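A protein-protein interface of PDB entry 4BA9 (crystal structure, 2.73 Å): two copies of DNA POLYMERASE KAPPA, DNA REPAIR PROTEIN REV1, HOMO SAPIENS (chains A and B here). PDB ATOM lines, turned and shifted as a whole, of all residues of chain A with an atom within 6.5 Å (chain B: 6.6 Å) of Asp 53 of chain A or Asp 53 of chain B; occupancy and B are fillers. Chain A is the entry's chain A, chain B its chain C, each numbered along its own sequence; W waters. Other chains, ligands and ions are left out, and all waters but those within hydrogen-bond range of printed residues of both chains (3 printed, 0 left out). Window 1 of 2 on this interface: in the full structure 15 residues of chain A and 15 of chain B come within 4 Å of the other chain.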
ATOM      1  N   LYS A   6     -18.475  16.532  -8.308  1.00  0.00           N
ATOM      2  CA  LYS A   6     -17.567  15.836  -7.420  1.00  0.00           C
ATOM      3  C   LYS A   6     -17.959  16.228  -5.991  1.00  0.00           C
ATOM      4  O   LYS A   6     -17.628  17.325  -5.547  1.00  0.00           O
ATOM      5  CB  LYS A   6     -16.090  16.196  -7.748  1.00  0.00           C
ATOM      6  CG  LYS A   6     -15.652  15.855  -9.174  1.00  0.00           C
ATOM      7  CD  LYS A   6     -14.209  15.373  -9.285  1.00  0.00           C
ATOM      8  CE  LYS A   6     -14.063  14.541 -10.540  1.00  0.00           C
ATOM      9  NZ  LYS A   6     -12.774  13.800 -10.588  1.00  0.00           N
ATOM     10  N   TRP A  47     -17.642   4.961   3.466  1.00  0.00           N
ATOM     11  CA  TRP A  47     -16.954   5.546   2.325  1.00  0.00           C
ATOM     12  C   TRP A  47     -16.625   4.479   1.272  1.00  0.00           C
ATOM     13  O   TRP A  47     -17.065   4.610   0.131  1.00  0.00           O
ATOM     14  CB  TRP A  47     -15.679   6.286   2.780  1.00  0.00           C
ATOM     15  CG  TRP A  47     -14.936   7.021   1.702  1.00  0.00           C
ATOM     16  CD1 TRP A  47     -15.466   7.833   0.740  1.00  0.00           C
ATOM     17  CD2 TRP A  47     -13.512   7.085   1.543  1.00  0.00           C
ATOM     18  NE1 TRP A  47     -14.465   8.362  -0.038  1.00  0.00           N
ATOM     19  CE2 TRP A  47     -13.251   7.934   0.445  1.00  0.00           C
ATOM     20  CE3 TRP A  47     -12.425   6.504   2.226  1.00  0.00           C
ATOM     21  CZ2 TRP A  47     -11.950   8.208   0.004  1.00  0.00           C
ATOM     22  CZ3 TRP A  47     -11.139   6.785   1.795  1.00  0.00           C
ATOM     23  CH2 TRP A  47     -10.910   7.627   0.697  1.00  0.00           C
ATOM     24  N   ILE A  51     -19.375   4.464  -1.850  1.00  0.00           N
ATOM     25  CA  ILE A  51     -18.873   5.241  -2.983  1.00  0.00           C
ATOM     26  C   ILE A  51     -18.126   4.331  -3.953  1.00  0.00           C
ATOM     27  O   ILE A  51     -17.335   3.481  -3.557  1.00  0.00           O
ATOM     28  CB  ILE A  51     -18.037   6.454  -2.493  1.00  0.00           C
ATOM     29  CG1 ILE A  51     -18.951   7.577  -1.984  1.00  0.00           C
ATOM     30  CG2 ILE A  51     -17.150   7.023  -3.581  1.00  0.00           C
ATOM     31  CD1 ILE A  51     -19.346   7.483  -0.600  1.00  0.00           C
ATOM     32  N   SER A  52     -18.425   4.498  -5.229  1.00  0.00           N
ATOM     33  CA  SER A  52     -17.843   3.711  -6.314  1.00  0.00           C
ATOM     34  C   SER A  52     -16.531   4.322  -6.806  1.00  0.00           C
ATOM     35  O   SER A  52     -15.620   3.566  -7.137  1.00  0.00           O
ATOM     36  CB  SER A  52     -18.835   3.573  -7.464  1.00  0.00           C
ATOM     37  OG  SER A  52     -19.507   4.803  -7.693  1.00  0.00           O
ATOM     38  N   ASP A  53     -16.451   5.676  -6.900  1.00  0.00           N
ATOM     39  CA  ASP A  53     -15.243   6.393  -7.312  1.00  0.00           C
ATOM     40  C   ASP A  53     -14.776   7.331  -6.181  1.00  0.00           C
ATOM     41  O   ASP A  53     -15.387   8.387  -5.989  1.00  0.00           O
ATOM     42  CB  ASP A  53     -15.439   7.186  -8.622  1.00  0.00           C
ATOM     43  CG  ASP A  53     -14.189   7.941  -9.129  1.00  0.00           C
ATOM     44  OD1 ASP A  53     -13.039   7.464  -8.868  1.00  0.00           O
ATOM     45  OD2 ASP A  53     -14.357   8.996  -9.803  1.00  0.00           O
ATOM     46  N   PRO A  54     -13.704   6.977  -5.427  1.00  0.00           N
ATOM     47  CA  PRO A  54     -13.220   7.894  -4.380  1.00  0.00           C
ATOM     48  C   PRO A  54     -12.692   9.210  -4.974  1.00  0.00           C
ATOM     49  O   PRO A  54     -12.035   9.221  -6.027  1.00  0.00           O
ATOM     50  CB  PRO A  54     -12.105   7.100  -3.698  1.00  0.00           C
ATOM     51  CG  PRO A  54     -11.652   6.110  -4.736  1.00  0.00           C
ATOM     52  CD  PRO A  54     -12.867   5.757  -5.518  1.00  0.00           C
ATOM     53  N   MET A  55     -13.007  10.317  -4.309  1.00  0.00           N
ATOM     54  CA  MET A  55     -12.587  11.646  -4.720  1.00  0.00           C
ATOM     55  C   MET A  55     -11.225  11.990  -4.159  1.00  0.00           C
ATOM     56  O   MET A  55     -10.941  11.663  -2.995  1.00  0.00           O
ATOM     57  CB  MET A  55     -13.598  12.667  -4.221  1.00  0.00           C
ATOM     58  CG  MET A  55     -14.576  13.105  -5.255  1.00  0.00           C
ATOM     59  SD  MET A  55     -15.640  14.289  -4.442  1.00  0.00           S
ATOM     60  CE  MET A  55     -14.450  15.566  -3.927  1.00  0.00           C
ATOM     61  N   VAL A  96      -9.738   1.474  -8.560  1.00  0.00           N
ATOM     62  CA  VAL A  96      -9.686   2.825  -7.994  1.00  0.00           C
ATOM     63  C   VAL A  96      -9.498   2.770  -6.483  1.00  0.00           C
ATOM     64  O   VAL A  96      -8.797   3.614  -5.939  1.00  0.00           O
ATOM     65  CB  VAL A  96     -10.911   3.701  -8.366  1.00  0.00           C
ATOM     66  CG1 VAL A  96     -10.821   4.183  -9.808  1.00  0.00           C
ATOM     67  CG2 VAL A  96     -12.239   2.988  -8.102  1.00  0.00           C
ATOM     68  N   TRP A  97     -10.099   1.780  -5.811  1.00  0.00           N
ATOM     69  CA  TRP A  97      -9.976   1.663  -4.365  1.00  0.00           C
ATOM     70  C   TRP A  97      -8.660   1.011  -3.986  1.00  0.00           C
ATOM     71  O   TRP A  97      -8.115   1.302  -2.922  1.00  0.00           O
ATOM     72  CB  TRP A  97     -11.155   0.904  -3.780  1.00  0.00           C
ATOM     73  CG  TRP A  97     -12.378   1.757  -3.635  1.00  0.00           C
ATOM     74  CD1 TRP A  97     -13.510   1.700  -4.394  1.00  0.00           C
ATOM     75  CD2 TRP A  97     -12.567   2.830  -2.709  1.00  0.00           C
ATOM     76  NE1 TRP A  97     -14.417   2.632  -3.959  1.00  0.00           N
ATOM     77  CE2 TRP A  97     -13.862   3.347  -2.930  1.00  0.00           C
ATOM     78  CE3 TRP A  97     -11.781   3.386  -1.680  1.00  0.00           C
ATOM     79  CZ2 TRP A  97     -14.394   4.392  -2.161  1.00  0.00           C
ATOM     80  CZ3 TRP A  97     -12.309   4.421  -0.917  1.00  0.00           C
ATOM     81  CH2 TRP A  97     -13.602   4.910  -1.157  1.00  0.00           C
ATOM     82  N   MET A  99      -5.829   1.369  -5.798  1.00  0.00           N
ATOM     83  CA  MET A  99      -4.910   2.476  -6.054  1.00  0.00           C
ATOM     84  C   MET A  99      -5.007   3.553  -4.965  1.00  0.00           C
ATOM     85  O   MET A  99      -3.973   4.105  -4.579  1.00  0.00           O
ATOM     86  CB  MET A  99      -5.181   3.095  -7.417  1.00  0.00           C
ATOM     87  CG  MET A  99      -4.819   2.185  -8.575  1.00  0.00           C
ATOM     88  SD  MET A  99      -4.940   3.011 -10.179  1.00  0.00           S
ATOM     89  CE  MET A  99      -6.719   3.290 -10.276  1.00  0.00           C
ATOM     90  N   TRP B  47      -7.977   4.694 -24.966  1.00  0.00           N
ATOM     91  CA  TRP B  47      -8.408   5.305 -23.702  1.00  0.00           C
ATOM     92  C   TRP B  47      -9.055   4.309 -22.719  1.00  0.00           C
ATOM     93  O   TRP B  47      -8.587   4.198 -21.585  1.00  0.00           O
ATOM     94  CB  TRP B  47      -9.381   6.483 -23.950  1.00  0.00           C
ATOM     95  CG  TRP B  47      -9.774   7.278 -22.721  1.00  0.00           C
ATOM     96  CD1 TRP B  47      -8.951   7.708 -21.715  1.00  0.00           C
ATOM     97  CD2 TRP B  47     -11.086   7.784 -22.410  1.00  0.00           C
ATOM     98  NE1 TRP B  47      -9.682   8.380 -20.757  1.00  0.00           N
ATOM     99  CE2 TRP B  47     -10.994   8.452 -21.164  1.00  0.00           C
ATOM    100  CE3 TRP B  47     -12.346   7.693 -23.038  1.00  0.00           C
ATOM    101  CZ2 TRP B  47     -12.110   9.038 -20.546  1.00  0.00           C
ATOM    102  CZ3 TRP B  47     -13.448   8.253 -22.413  1.00  0.00           C
ATOM    103  CH2 TRP B  47     -13.325   8.921 -21.188  1.00  0.00           C
ATOM    104  N   THR B  50      -6.459   1.352 -21.537  1.00  0.00           N
ATOM    105  CA  THR B  50      -5.259   1.759 -20.769  1.00  0.00           C
ATOM    106  C   THR B  50      -5.557   2.384 -19.383  1.00  0.00           C
ATOM    107  O   THR B  50      -4.965   1.980 -18.375  1.00  0.00           O
ATOM    108  CB  THR B  50      -4.466   2.800 -21.607  1.00  0.00           C
ATOM    109  OG1 THR B  50      -4.161   2.296 -22.916  1.00  0.00           O
ATOM    110  CG2 THR B  50      -3.212   3.316 -20.910  1.00  0.00           C
ATOM    111  N   ILE B  51      -6.421   3.413 -19.361  1.00  0.00           N
ATOM    112  CA  ILE B  51      -6.762   4.234 -18.188  1.00  0.00           C
ATOM    113  C   ILE B  51      -7.778   3.535 -17.264  1.00  0.00           C
ATOM    114  O   ILE B  51      -8.880   3.208 -17.687  1.00  0.00           O
ATOM    115  CB  ILE B  51      -7.256   5.622 -18.678  1.00  0.00           C
ATOM    116  CG1 ILE B  51      -6.095   6.417 -19.337  1.00  0.00           C
ATOM    117  CG2 ILE B  51      -7.876   6.437 -17.563  1.00  0.00           C
ATOM    118  CD1 ILE B  51      -5.891   6.185 -20.831  1.00  0.00           C
ATOM    119  N   SER B  52      -7.388   3.346 -15.995  1.00  0.00           N
ATOM    120  CA  SER B  52      -8.168   2.679 -14.939  1.00  0.00           C
ATOM    121  C   SER B  52      -9.235   3.585 -14.264  1.00  0.00           C
ATOM    122  O   SER B  52     -10.208   3.065 -13.701  1.00  0.00           O
ATOM    123  CB  SER B  52      -7.231   2.121 -13.871  1.00  0.00           C
ATOM    124  OG  SER B  52      -6.192   3.039 -13.567  1.00  0.00           O
ATOM    125  N   ASP B  53      -9.029   4.918 -14.291  1.00  0.00           N
ATOM    126  CA  ASP B  53      -9.943   5.919 -13.733  1.00  0.00           C
ATOM    127  C   ASP B  53     -10.085   7.030 -14.770  1.00  0.00           C
ATOM    128  O   ASP B  53      -9.115   7.772 -14.978  1.00  0.00           O
ATOM    129  CB  ASP B  53      -9.426   6.454 -12.374  1.00  0.00           C
ATOM    130  CG  ASP B  53     -10.278   7.514 -11.672  1.00  0.00           C
ATOM    131  OD1 ASP B  53     -11.268   8.002 -12.289  1.00  0.00           O
ATOM    132  OD2 ASP B  53      -9.949   7.867 -10.506  1.00  0.00           O
ATOM    133  N   PRO B  54     -11.240   7.158 -15.474  1.00  0.00           N
ATOM    134  CA  PRO B  54     -11.355   8.242 -16.465  1.00  0.00           C
ATOM    135  C   PRO B  54     -11.492   9.609 -15.774  1.00  0.00           C
ATOM    136  O   PRO B  54     -12.090   9.730 -14.681  1.00  0.00           O
ATOM    137  CB  PRO B  54     -12.598   7.861 -17.291  1.00  0.00           C
ATOM    138  CG  PRO B  54     -13.136   6.634 -16.699  1.00  0.00           C
ATOM    139  CD  PRO B  54     -12.500   6.400 -15.375  1.00  0.00           C
ATOM    140  N   MET B  55     -10.895  10.622 -16.408  1.00  0.00           N
ATOM    141  CA  MET B  55     -10.896  12.007 -15.944  1.00  0.00           C
ATOM    142  C   MET B  55     -12.100  12.737 -16.527  1.00  0.00           C
ATOM    143  O   MET B  55     -12.458  12.513 -17.697  1.00  0.00           O
ATOM    144  CB  MET B  55      -9.583  12.681 -16.388  1.00  0.00           C
ATOM    145  CG  MET B  55      -9.229  13.947 -15.659  1.00  0.00           C
ATOM    146  SD  MET B  55      -7.719  14.615 -16.380  1.00  0.00           S
ATOM    147  CE  MET B  55      -7.793  16.293 -15.774  1.00  0.00           C
ATOM    148  N   SER B  95     -16.660  -0.005 -12.476  1.00  0.00           N
ATOM    149  CA  SER B  95     -17.890   0.791 -12.354  1.00  0.00           C
ATOM    150  C   SER B  95     -17.707   2.211 -12.881  1.00  0.00           C
ATOM    151  O   SER B  95     -18.631   2.761 -13.459  1.00  0.00           O
ATOM    152  CB  SER B  95     -18.358   0.837 -10.907  1.00  0.00           C
ATOM    153  OG  SER B  95     -18.530  -0.484 -10.421  1.00  0.00           O
ATOM    154  N   VAL B  96     -16.503   2.778 -12.718  1.00  0.00           N
ATOM    155  CA  VAL B  96     -16.127   4.111 -13.196  1.00  0.00           C
ATOM    156  C   VAL B  96     -16.337   4.234 -14.706  1.00  0.00           C
ATOM    157  O   VAL B  96     -16.746   5.299 -15.173  1.00  0.00           O
ATOM    158  CB  VAL B  96     -14.682   4.521 -12.812  1.00  0.00           C
ATOM    159  CG1 VAL B  96     -14.601   4.887 -11.342  1.00  0.00           C
ATOM    160  CG2 VAL B  96     -13.652   3.447 -13.173  1.00  0.00           C
ATOM    161  N   TRP B  97     -16.080   3.149 -15.463  1.00  0.00           N
ATOM    162  CA  TRP B  97     -16.253   3.170 -16.908  1.00  0.00           C
ATOM    163  C   TRP B  97     -17.705   2.976 -17.277  1.00  0.00           C
ATOM    164  O   TRP B  97     -18.135   3.479 -18.314  1.00  0.00           O
ATOM    165  CB  TRP B  97     -15.376   2.125 -17.569  1.00  0.00           C
ATOM    166  CG  TRP B  97     -13.960   2.582 -17.706  1.00  0.00           C
ATOM    167  CD1 TRP B  97     -12.886   2.136 -17.000  1.00  0.00           C
ATOM    168  CD2 TRP B  97     -13.466   3.613 -18.581  1.00  0.00           C
ATOM    169  NE1 TRP B  97     -11.747   2.796 -17.403  1.00  0.00           N
ATOM    170  CE2 TRP B  97     -12.076   3.708 -18.373  1.00  0.00           C
ATOM    171  CE3 TRP B  97     -14.067   4.451 -19.544  1.00  0.00           C
ATOM    172  CZ2 TRP B  97     -11.271   4.603 -19.091  1.00  0.00           C
ATOM    173  CZ3 TRP B  97     -13.271   5.336 -20.255  1.00  0.00           C
ATOM    174  CH2 TRP B  97     -11.891   5.412 -20.021  1.00  0.00           C
ATOM    175  N   MET B  99     -20.250   4.092 -15.357  1.00  0.00           N
ATOM    176  CA  MET B  99     -20.777   5.416 -15.015  1.00  0.00           C
ATOM    177  C   MET B  99     -20.368   6.466 -16.049  1.00  0.00           C
ATOM    178  O   MET B  99     -21.178   7.321 -16.383  1.00  0.00           O
ATOM    179  CB  MET B  99     -20.325   5.837 -13.625  1.00  0.00           C
ATOM    180  CG  MET B  99     -20.945   5.006 -12.516  1.00  0.00           C
ATOM    181  SD  MET B  99     -20.553   5.656 -10.881  1.00  0.00           S
ATOM    182  CE  MET B  99     -18.777   5.335 -10.809  1.00  0.00           C
HETATM  183  O   HOH W   1      -9.366   9.072  -7.726  1.00  0.00           O
HETATM  184  O   HOH W   2     -11.195   1.457 -11.429  1.00  0.00           O
HETATM  185  O   HOH W   3     -11.910  10.115  -9.812  1.00  0.00           O
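Printed residues of chain A that touch a printed residue of chain B: Ser 52, Asp 53, Val 96 and Met 99. Among the printed residues, no Asp or Glu carboxylate lies within 4 Å of a Lys or Arg side-chain nitrogen of the other chain.
Water W3 lies within hydrogen-bond range of the side-chain carboxylate (OD2) of Asp 53 of chain A (2.7 Å) and the side-chain carboxylate (OD2) of Asp 53 of chain B (3.1 Å). Water W2 bridges the backbone carbonyl oxygen of Ser 52 of chain B and the backbone NH of Val 96 of chain A. Water W1 bridges OD2 of Asp 53 of chain B (3.1 Å) and O of Pro 54 of chain A (3.2 Å).
Ser 52 of chain A touches Met 99 of chain B, and with the chains exchanged Met 99 of chain A touches Ser 52 of chain B. Asp 53 of chain B touches its own counterpart, Asp 53 of chain A. Asp 53 of chain A touches Val 96 of chain B, and with the chains exchanged Val 96 of chain A touches Asp 53 of chain B. Of the 5 pairs that touch across the chains among the printed residues, 5 have their exchanged pair printed and touching as well.
Asp 53 of chain A touches just these residues of chain B: Asp 53 and Val 96. Asp 53 of chain B touches just these residues of chain A: Asp 53 (3.5 Å) and Val 96 (3.7 Å). Of the printed residues of chain A, Ser 52 of chain B touches Met 99. Of the printed residues of chain A, Val 96 of chain B touches Asp 53 (3.7 Å). Of the printed residues of chain B, Met 99 of chain A touches Ser 52 (3.3 Å). Of the printed residues of chain B, Ser 52 of chain A touches Met 99 (3.2 Å). Of the printed residues of chain B, Val 96 of chain A touches Asp 53 (3.7 Å).
OD2 of Asp 53 of chain B touches OD1 of Asp 53 of chain A, at 3.5 Å. Asp 53 of chain A touches Val 96 of chain B (CB to CG1, 3.7 Å). Val 96 of chain A touches Asp 53 of chain B (CG1 to CB, 3.7 Å).
The side-chain hydroxyl of Ser 52 of chain A sits close to the side-chain sulfur of Met 99 of chain B, at 3.5 Å. The side-chain hydroxyl (OG) of Ser 52 of chain B lies close to the side-chain sulfur (SD) of Met 99 of chain A, at 3.6 Å.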
